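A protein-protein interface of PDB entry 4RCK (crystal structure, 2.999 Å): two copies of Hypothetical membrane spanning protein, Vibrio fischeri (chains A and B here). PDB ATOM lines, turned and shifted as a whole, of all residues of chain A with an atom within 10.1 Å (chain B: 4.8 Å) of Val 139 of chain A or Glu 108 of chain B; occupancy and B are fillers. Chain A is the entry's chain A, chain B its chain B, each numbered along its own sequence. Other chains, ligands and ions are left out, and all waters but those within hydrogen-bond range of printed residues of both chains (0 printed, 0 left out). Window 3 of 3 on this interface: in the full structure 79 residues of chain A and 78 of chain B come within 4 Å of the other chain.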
ATOM      1  N   ILE A 127     -10.267   2.780  34.142  1.00  0.00           N
ATOM      2  CA  ILE A 127      -9.533   1.672  33.542  1.00  0.00           C
ATOM      3  C   ILE A 127      -8.511   1.116  34.527  1.00  0.00           C
ATOM      4  O   ILE A 127      -7.799   1.872  35.183  1.00  0.00           O
ATOM      5  CB  ILE A 127      -8.806   2.098  32.247  1.00  0.00           C
ATOM      6  CG1 ILE A 127      -9.768   2.807  31.292  1.00  0.00           C
ATOM      7  CG2 ILE A 127      -8.168   0.893  31.568  1.00  0.00           C
ATOM      8  CD1 ILE A 127      -9.112   3.291  30.016  1.00  0.00           C
ATOM      9  N   LEU A 129      -5.308  -1.250  34.331  1.00  0.00           N
ATOM     10  CA  LEU A 129      -4.350  -1.969  33.502  1.00  0.00           C
ATOM     11  C   LEU A 129      -3.217  -2.540  34.339  1.00  0.00           C
ATOM     12  O   LEU A 129      -2.645  -1.843  35.177  1.00  0.00           O
ATOM     13  CB  LEU A 129      -3.781  -1.048  32.420  1.00  0.00           C
ATOM     14  CG  LEU A 129      -2.402  -1.376  31.840  1.00  0.00           C
ATOM     15  CD1 LEU A 129      -2.510  -2.394  30.717  1.00  0.00           C
ATOM     16  CD2 LEU A 129      -1.703  -0.108  31.365  1.00  0.00           C
ATOM     17  N   ASN A 135       5.793  -1.718  26.744  1.00  0.00           N
ATOM     18  CA  ASN A 135       5.022  -1.758  25.516  1.00  0.00           C
ATOM     19  C   ASN A 135       5.949  -2.013  24.329  1.00  0.00           C
ATOM     20  O   ASN A 135       6.335  -1.083  23.620  1.00  0.00           O
ATOM     21  CB  ASN A 135       4.241  -0.453  25.349  1.00  0.00           C
ATOM     22  CG  ASN A 135       3.540  -0.355  24.012  1.00  0.00           C
ATOM     23  OD1 ASN A 135       2.559  -1.051  23.760  1.00  0.00           O
ATOM     24  ND2 ASN A 135       4.045   0.513  23.144  1.00  0.00           N
ATOM     25  N   THR A 136       6.312  -3.279  24.130  1.00  0.00           N
ATOM     26  CA  THR A 136       7.300  -3.652  23.119  1.00  0.00           C
ATOM     27  C   THR A 136       6.772  -3.465  21.696  1.00  0.00           C
ATOM     28  O   THR A 136       7.459  -2.903  20.844  1.00  0.00           O
ATOM     29  CB  THR A 136       7.764  -5.122  23.290  1.00  0.00           C
ATOM     30  OG1 THR A 136       6.775  -6.007  22.756  1.00  0.00           O
ATOM     31  CG2 THR A 136       7.996  -5.456  24.760  1.00  0.00           C
ATOM     32  N   ALA A 137       5.549  -3.922  21.447  1.00  0.00           N
ATOM     33  CA  ALA A 137       4.971  -3.887  20.106  1.00  0.00           C
ATOM     34  C   ALA A 137       3.537  -3.379  20.098  1.00  0.00           C
ATOM     35  O   ALA A 137       2.731  -3.791  20.907  1.00  0.00           O
ATOM     36  CB  ALA A 137       5.024  -5.261  19.485  1.00  0.00           C
ATOM     37  N   GLY A 138       3.219  -2.513  19.145  1.00  0.00           N
ATOM     38  CA  GLY A 138       1.892  -1.935  19.039  1.00  0.00           C
ATOM     39  C   GLY A 138       1.926  -0.701  18.168  1.00  0.00           C
ATOM     40  O   GLY A 138       2.906   0.044  18.181  1.00  0.00           O
ATOM     41  N   VAL A 139       0.869  -0.486  17.394  1.00  0.00           N
ATOM     42  CA  VAL A 139       0.815   0.675  16.522  1.00  0.00           C
ATOM     43  C   VAL A 139       0.563   1.932  17.353  1.00  0.00           C
ATOM     44  O   VAL A 139       1.173   2.974  17.118  1.00  0.00           O
ATOM     45  CB  VAL A 139      -0.268   0.520  15.422  1.00  0.00           C
ATOM     46  CG1 VAL A 139      -1.387  -0.392  15.883  1.00  0.00           C
ATOM     47  CG2 VAL A 139      -0.802   1.880  14.987  1.00  0.00           C
ATOM     48  N   LEU A 140      -0.333   1.823  18.329  1.00  0.00           N
ATOM     49  CA  LEU A 140      -0.652   2.952  19.197  1.00  0.00           C
ATOM     50  C   LEU A 140       0.306   3.013  20.382  1.00  0.00           C
ATOM     51  O   LEU A 140       0.454   2.041  21.123  1.00  0.00           O
ATOM     52  CB  LEU A 140      -2.097   2.862  19.694  1.00  0.00           C
ATOM     53  CG  LEU A 140      -2.957   4.124  19.575  1.00  0.00           C
ATOM     54  CD1 LEU A 140      -4.181   4.024  20.475  1.00  0.00           C
ATOM     55  CD2 LEU A 140      -2.155   5.379  19.888  1.00  0.00           C
ATOM     56  N   GLU A 141       0.953   4.161  20.554  1.00  0.00           N
ATOM     57  CA  GLU A 141       1.875   4.365  21.667  1.00  0.00           C
ATOM     58  C   GLU A 141       1.113   4.513  22.981  1.00  0.00           C
ATOM     59  O   GLU A 141      -0.024   4.982  22.988  1.00  0.00           O
ATOM     60  CB  GLU A 141       2.755   5.594  21.417  1.00  0.00           C
ATOM     61  CG  GLU A 141       3.819   5.375  20.360  1.00  0.00           C
ATOM     62  CD  GLU A 141       4.683   4.164  20.659  1.00  0.00           C
ATOM     63  OE1 GLU A 141       5.250   4.093  21.769  1.00  0.00           O
ATOM     64  OE2 GLU A 141       4.787   3.279  19.785  1.00  0.00           O
ATOM     65  N   PRO A 142       1.738   4.103  24.100  1.00  0.00           N
ATOM     66  CA  PRO A 142       1.104   4.138  25.425  1.00  0.00           C
ATOM     67  C   PRO A 142       0.601   5.518  25.836  1.00  0.00           C
ATOM     68  O   PRO A 142      -0.528   5.640  26.316  1.00  0.00           O
ATOM     69  CB  PRO A 142       2.230   3.687  26.360  1.00  0.00           C
ATOM     70  CG  PRO A 142       3.124   2.878  25.509  1.00  0.00           C
ATOM     71  CD  PRO A 142       3.087   3.515  24.156  1.00  0.00           C
ATOM     72  N   LEU A 143       1.433   6.539  25.656  1.00  0.00           N
ATOM     73  CA  LEU A 143       1.106   7.882  26.121  1.00  0.00           C
ATOM     74  C   LEU A 143       0.159   8.586  25.174  1.00  0.00           C
ATOM     75  O   LEU A 143      -0.533   9.524  25.556  1.00  0.00           O
ATOM     76  CB  LEU A 143       2.374   8.710  26.295  1.00  0.00           C
ATOM     77  CG  LEU A 143       3.285   8.175  27.393  1.00  0.00           C
ATOM     78  CD1 LEU A 143       4.495   9.071  27.566  1.00  0.00           C
ATOM     79  CD2 LEU A 143       2.510   8.043  28.695  1.00  0.00           C
ATOM     80  N   GLU A 144       0.138   8.143  23.927  1.00  0.00           N
ATOM     81  CA  GLU A 144      -0.906   8.594  23.038  1.00  0.00           C
ATOM     82  C   GLU A 144      -2.208   8.017  23.566  1.00  0.00           C
ATOM     83  O   GLU A 144      -3.139   8.757  23.871  1.00  0.00           O
ATOM     84  CB  GLU A 144      -0.651   8.155  21.607  1.00  0.00           C
ATOM     85  CG  GLU A 144       0.716   8.510  21.081  1.00  0.00           C
ATOM     86  CD  GLU A 144       0.843   8.136  19.632  1.00  0.00           C
ATOM     87  OE1 GLU A 144       1.976   7.908  19.159  1.00  0.00           O
ATOM     88  OE2 GLU A 144      -0.213   8.065  18.972  1.00  0.00           O
ATOM     89  N   ALA A 145      -2.243   6.693  23.706  1.00  0.00           N
ATOM     90  CA  ALA A 145      -3.417   5.982  24.209  1.00  0.00           C
ATOM     91  C   ALA A 145      -3.890   6.515  25.556  1.00  0.00           C
ATOM     92  O   ALA A 145      -5.088   6.543  25.835  1.00  0.00           O
ATOM     93  CB  ALA A 145      -3.126   4.498  24.313  1.00  0.00           C
ATOM     94  N   ALA A 146      -2.942   6.928  26.389  1.00  0.00           N
ATOM     95  CA  ALA A 146      -3.268   7.518  27.681  1.00  0.00           C
ATOM     96  C   ALA A 146      -3.949   8.874  27.514  1.00  0.00           C
ATOM     97  O   ALA A 146      -4.895   9.198  28.238  1.00  0.00           O
ATOM     98  CB  ALA A 146      -2.012   7.656  28.533  1.00  0.00           C
ATOM     99  N   LEU A 148      -5.803   9.931  25.208  1.00  0.00           N
ATOM    100  CA  LEU A 148      -7.145   9.763  24.695  1.00  0.00           C
ATOM    101  C   LEU A 148      -8.116   9.399  25.798  1.00  0.00           C
ATOM    102  O   LEU A 148      -9.236   9.892  25.820  1.00  0.00           O
ATOM    103  CB  LEU A 148      -7.136   8.694  23.616  1.00  0.00           C
ATOM    104  CG  LEU A 148      -5.969   8.940  22.654  1.00  0.00           C
ATOM    105  CD1 LEU A 148      -5.526   7.727  22.008  1.00  0.00           C
ATOM    106  CD2 LEU A 148      -6.235  10.025  21.644  1.00  0.00           C
ATOM    107  N   ILE A 191       1.318   7.110  32.524  1.00  0.00           N
ATOM    108  CA  ILE A 191      -0.051   6.821  32.112  1.00  0.00           C
ATOM    109  C   ILE A 191      -1.050   7.147  33.218  1.00  0.00           C
ATOM    110  O   ILE A 191      -2.004   7.896  33.004  1.00  0.00           O
ATOM    111  CB  ILE A 191      -0.220   5.344  31.708  1.00  0.00           C
ATOM    112  CG1 ILE A 191       0.625   5.028  30.472  1.00  0.00           C
ATOM    113  CG2 ILE A 191      -1.682   5.027  31.444  1.00  0.00           C
ATOM    114  CD1 ILE A 191       0.531   3.586  30.020  1.00  0.00           C
ATOM    115  N   ASP B  73       0.657  -8.923  21.558  1.00  0.00           N
ATOM    116  CA  ASP B  73       0.835  -8.652  20.123  1.00  0.00           C
ATOM    117  C   ASP B  73      -0.364  -7.869  19.624  1.00  0.00           C
ATOM    118  O   ASP B  73      -0.283  -6.680  19.296  1.00  0.00           O
ATOM    119  CB  ASP B  73       0.952  -9.944  19.291  1.00  0.00           C
ATOM    120  CG  ASP B  73       2.190 -10.757  19.607  1.00  0.00           C
ATOM    121  OD1 ASP B  73       3.033 -10.298  20.403  1.00  0.00           O
ATOM    122  OD2 ASP B  73       2.312 -11.869  19.047  1.00  0.00           O
ATOM    123  N   ALA B  75      -4.352  -6.761  20.619  1.00  0.00           N
ATOM    124  CA  ALA B  75      -5.223  -6.583  21.770  1.00  0.00           C
ATOM    125  C   ALA B  75      -6.662  -6.809  21.340  1.00  0.00           C
ATOM    126  O   ALA B  75      -7.121  -6.224  20.356  1.00  0.00           O
ATOM    127  CB  ALA B  75      -5.051  -5.204  22.375  1.00  0.00           C
ATOM    128  N   ALA B 105       1.072  -5.061  23.401  1.00  0.00           N
ATOM    129  CA  ALA B 105       0.561  -3.770  22.965  1.00  0.00           C
ATOM    130  C   ALA B 105      -0.218  -3.100  24.072  1.00  0.00           C
ATOM    131  O   ALA B 105      -1.405  -3.363  24.251  1.00  0.00           O
ATOM    132  CB  ALA B 105      -0.307  -3.927  21.722  1.00  0.00           C
ATOM    133  N   ILE B 106       0.459  -2.236  24.817  1.00  0.00           N
ATOM    134  CA  ILE B 106      -0.183  -1.528  25.912  1.00  0.00           C
ATOM    135  C   ILE B 106      -1.083  -0.418  25.376  1.00  0.00           C
ATOM    136  O   ILE B 106      -2.227  -0.277  25.807  1.00  0.00           O
ATOM    137  CB  ILE B 106       0.856  -0.950  26.893  1.00  0.00           C
ATOM    138  CG1 ILE B 106       1.652  -2.087  27.533  1.00  0.00           C
ATOM    139  CG2 ILE B 106       0.177  -0.113  27.963  1.00  0.00           C
ATOM    140  CD1 ILE B 106       2.621  -1.644  28.606  1.00  0.00           C
ATOM    141  N   GLY B 107      -0.569   0.352  24.421  1.00  0.00           N
ATOM    142  CA  GLY B 107      -1.350   1.396  23.781  1.00  0.00           C
ATOM    143  C   GLY B 107      -2.595   0.862  23.093  1.00  0.00           C
ATOM    144  O   GLY B 107      -3.644   1.506  23.103  1.00  0.00           O
ATOM    145  N   GLU B 108      -2.477  -0.319  22.495  1.00  0.00           N
ATOM    146  CA  GLU B 108      -3.611  -0.971  21.847  1.00  0.00           C
ATOM    147  C   GLU B 108      -4.710  -1.281  22.850  1.00  0.00           C
ATOM    148  O   GLU B 108      -5.879  -0.970  22.621  1.00  0.00           O
ATOM    149  CB  GLU B 108      -3.172  -2.266  21.167  1.00  0.00           C
ATOM    150  CG  GLU B 108      -3.744  -2.498  19.789  1.00  0.00           C
ATOM    151  CD  GLU B 108      -2.872  -1.903  18.709  1.00  0.00           C
ATOM    152  OE1 GLU B 108      -2.371  -2.671  17.861  1.00  0.00           O
ATOM    153  OE2 GLU B 108      -2.685  -0.669  18.715  1.00  0.00           O
ATOM    154  N   GLY B 109      -4.321  -1.906  23.955  1.00  0.00           N
ATOM    155  CA  GLY B 109      -5.262  -2.301  24.985  1.00  0.00           C
ATOM    156  C   GLY B 109      -5.997  -1.123  25.593  1.00  0.00           C
ATOM    157  O   GLY B 109      -7.217  -1.160  25.755  1.00  0.00           O
ATOM    158  N   LEU B 110      -5.251  -0.074  25.925  1.00  0.00           N
ATOM    159  CA  LEU B 110      -5.832   1.123  26.522  1.00  0.00           C
ATOM    160  C   LEU B 110      -6.782   1.818  25.554  1.00  0.00           C
ATOM    161  O   LEU B 110      -7.818   2.345  25.959  1.00  0.00           O
ATOM    162  CB  LEU B 110      -4.731   2.089  26.965  1.00  0.00           C
ATOM    163  CG  LEU B 110      -3.809   1.567  28.067  1.00  0.00           C
ATOM    164  CD1 LEU B 110      -2.779   2.616  28.463  1.00  0.00           C
ATOM    165  CD2 LEU B 110      -4.621   1.123  29.272  1.00  0.00           C
ATOM    166  N   GLY B 111      -6.425   1.812  24.275  1.00  0.00           N
ATOM    167  CA  GLY B 111      -7.271   2.392  23.251  1.00  0.00           C
ATOM    168  C   GLY B 111      -8.558   1.612  23.077  1.00  0.00           C
ATOM    169  O   GLY B 111      -9.642   2.194  23.017  1.00  0.00           O
ATOM    170  N   LEU B 112      -8.439   0.289  23.000  1.00  0.00           N
ATOM    171  CA  LEU B 112      -9.598  -0.575  22.809  1.00  0.00           C
ATOM    172  C   LEU B 112     -10.553  -0.480  23.995  1.00  0.00           C
ATOM    173  O   LEU B 112     -11.771  -0.551  23.828  1.00  0.00           O
ATOM    174  CB  LEU B 112      -9.162  -2.027  22.594  1.00  0.00           C
ATOM    175  CG  LEU B 112     -10.284  -2.993  22.208  1.00  0.00           C
ATOM    176  CD1 LEU B 112     -11.010  -2.492  20.971  1.00  0.00           C
ATOM    177  CD2 LEU B 112      -9.747  -4.397  21.983  1.00  0.00           C
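The backbone carbonyl oxygen (O) of Ala 137 of chain A sits close to the backbone NH (N) of Ala 105 of chain B (3.3 Å).
The backbone NH (N) of Gly 107 of chain B sits at hydrogen-bond distance from the side-chain amide oxygen (OD1) of Asn 135 of chain A (3.5 Å).
The side-chain amide oxygen (OD1) of Asn 135 of chain A lies within hydrogen-bond range of the backbone NH (N) of Ile 106 of chain B (2.6 Å).
N of Leu 140 of chain A lies within hydrogen-bond range of OE2 of Glu 108 of chain B, 3.4 Å away.
Printed residues of chain B that touch a printed residue of chain A: Ala 105, Ile 106, Gly 107, Glu 108 and Leu 110.
Among the printed residues, 13 pairs touch across the chains.
Among the printed residues, no Asp or Glu carboxylate lies within 4 Å of a Lys or Arg side-chain nitrogen of the other chain.
Of chain B, only Glu 108 (3.1 Å) comes within 4 Å of Val 139 of chain A.
Printed residues of chain A within 4 Å of Glu 108 of chain B: Val 139 and Leu 140.
No residue of chain A comes within 4 Å of Ala 75 of chain B.
No residue of chain A comes within 4 Å of Gly 109 of chain B.
Gly 111 of chain B touches none of the printed residues of chain A.
No residue of chain A comes within 4 Å of Leu 112 of chain B.
Of the printed residues of chain B, Ile 191 of chain A touches Leu 110.
Of the printed residues of chain A, Ile 106 of chain B touches Leu 129 (3.9 Å) and Asn 135 (2.6 Å).
Printed residues of chain B within 4 Å of Asn 135 of chain A: Ala 105, Ile 106 and Gly 107.
Of the printed residues of chain A, Leu 110 of chain B touches Leu 129, Ala 145 and Ile 191.
Printed residues of chain B within 4 Å of Leu 129 of chain A: Ile 106 and Leu 110.
Ile 127 of chain A touches none of the printed residues of chain B.
Thr 136 of chain A touches none of the printed residues of chain B.
The nearest printed residue of chain B that does not touch Val 139 of chain A is Ala 105 of chain B (5.7 Å).
No position is printed for both chains.
Among the printed residues, pairs that only touch across the chains: Val 139 of chain A with Glu 108 of chain B, Ala 145 of chain A with Gly 107 of chain B, Leu 140 of chain A with Gly 107 of chain B, Asn 135 of chain A with Ala 105 of chain B, Ile 191 of chain A with Leu 110 of chain B, Leu 129 of chain A with Leu 110 of chain B, Leu 129 of chain A with Ile 106 of chain B, Glu 141 of chain A with Gly 107 of chain B and Ala 145 of chain A with Leu 110 of chain B.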
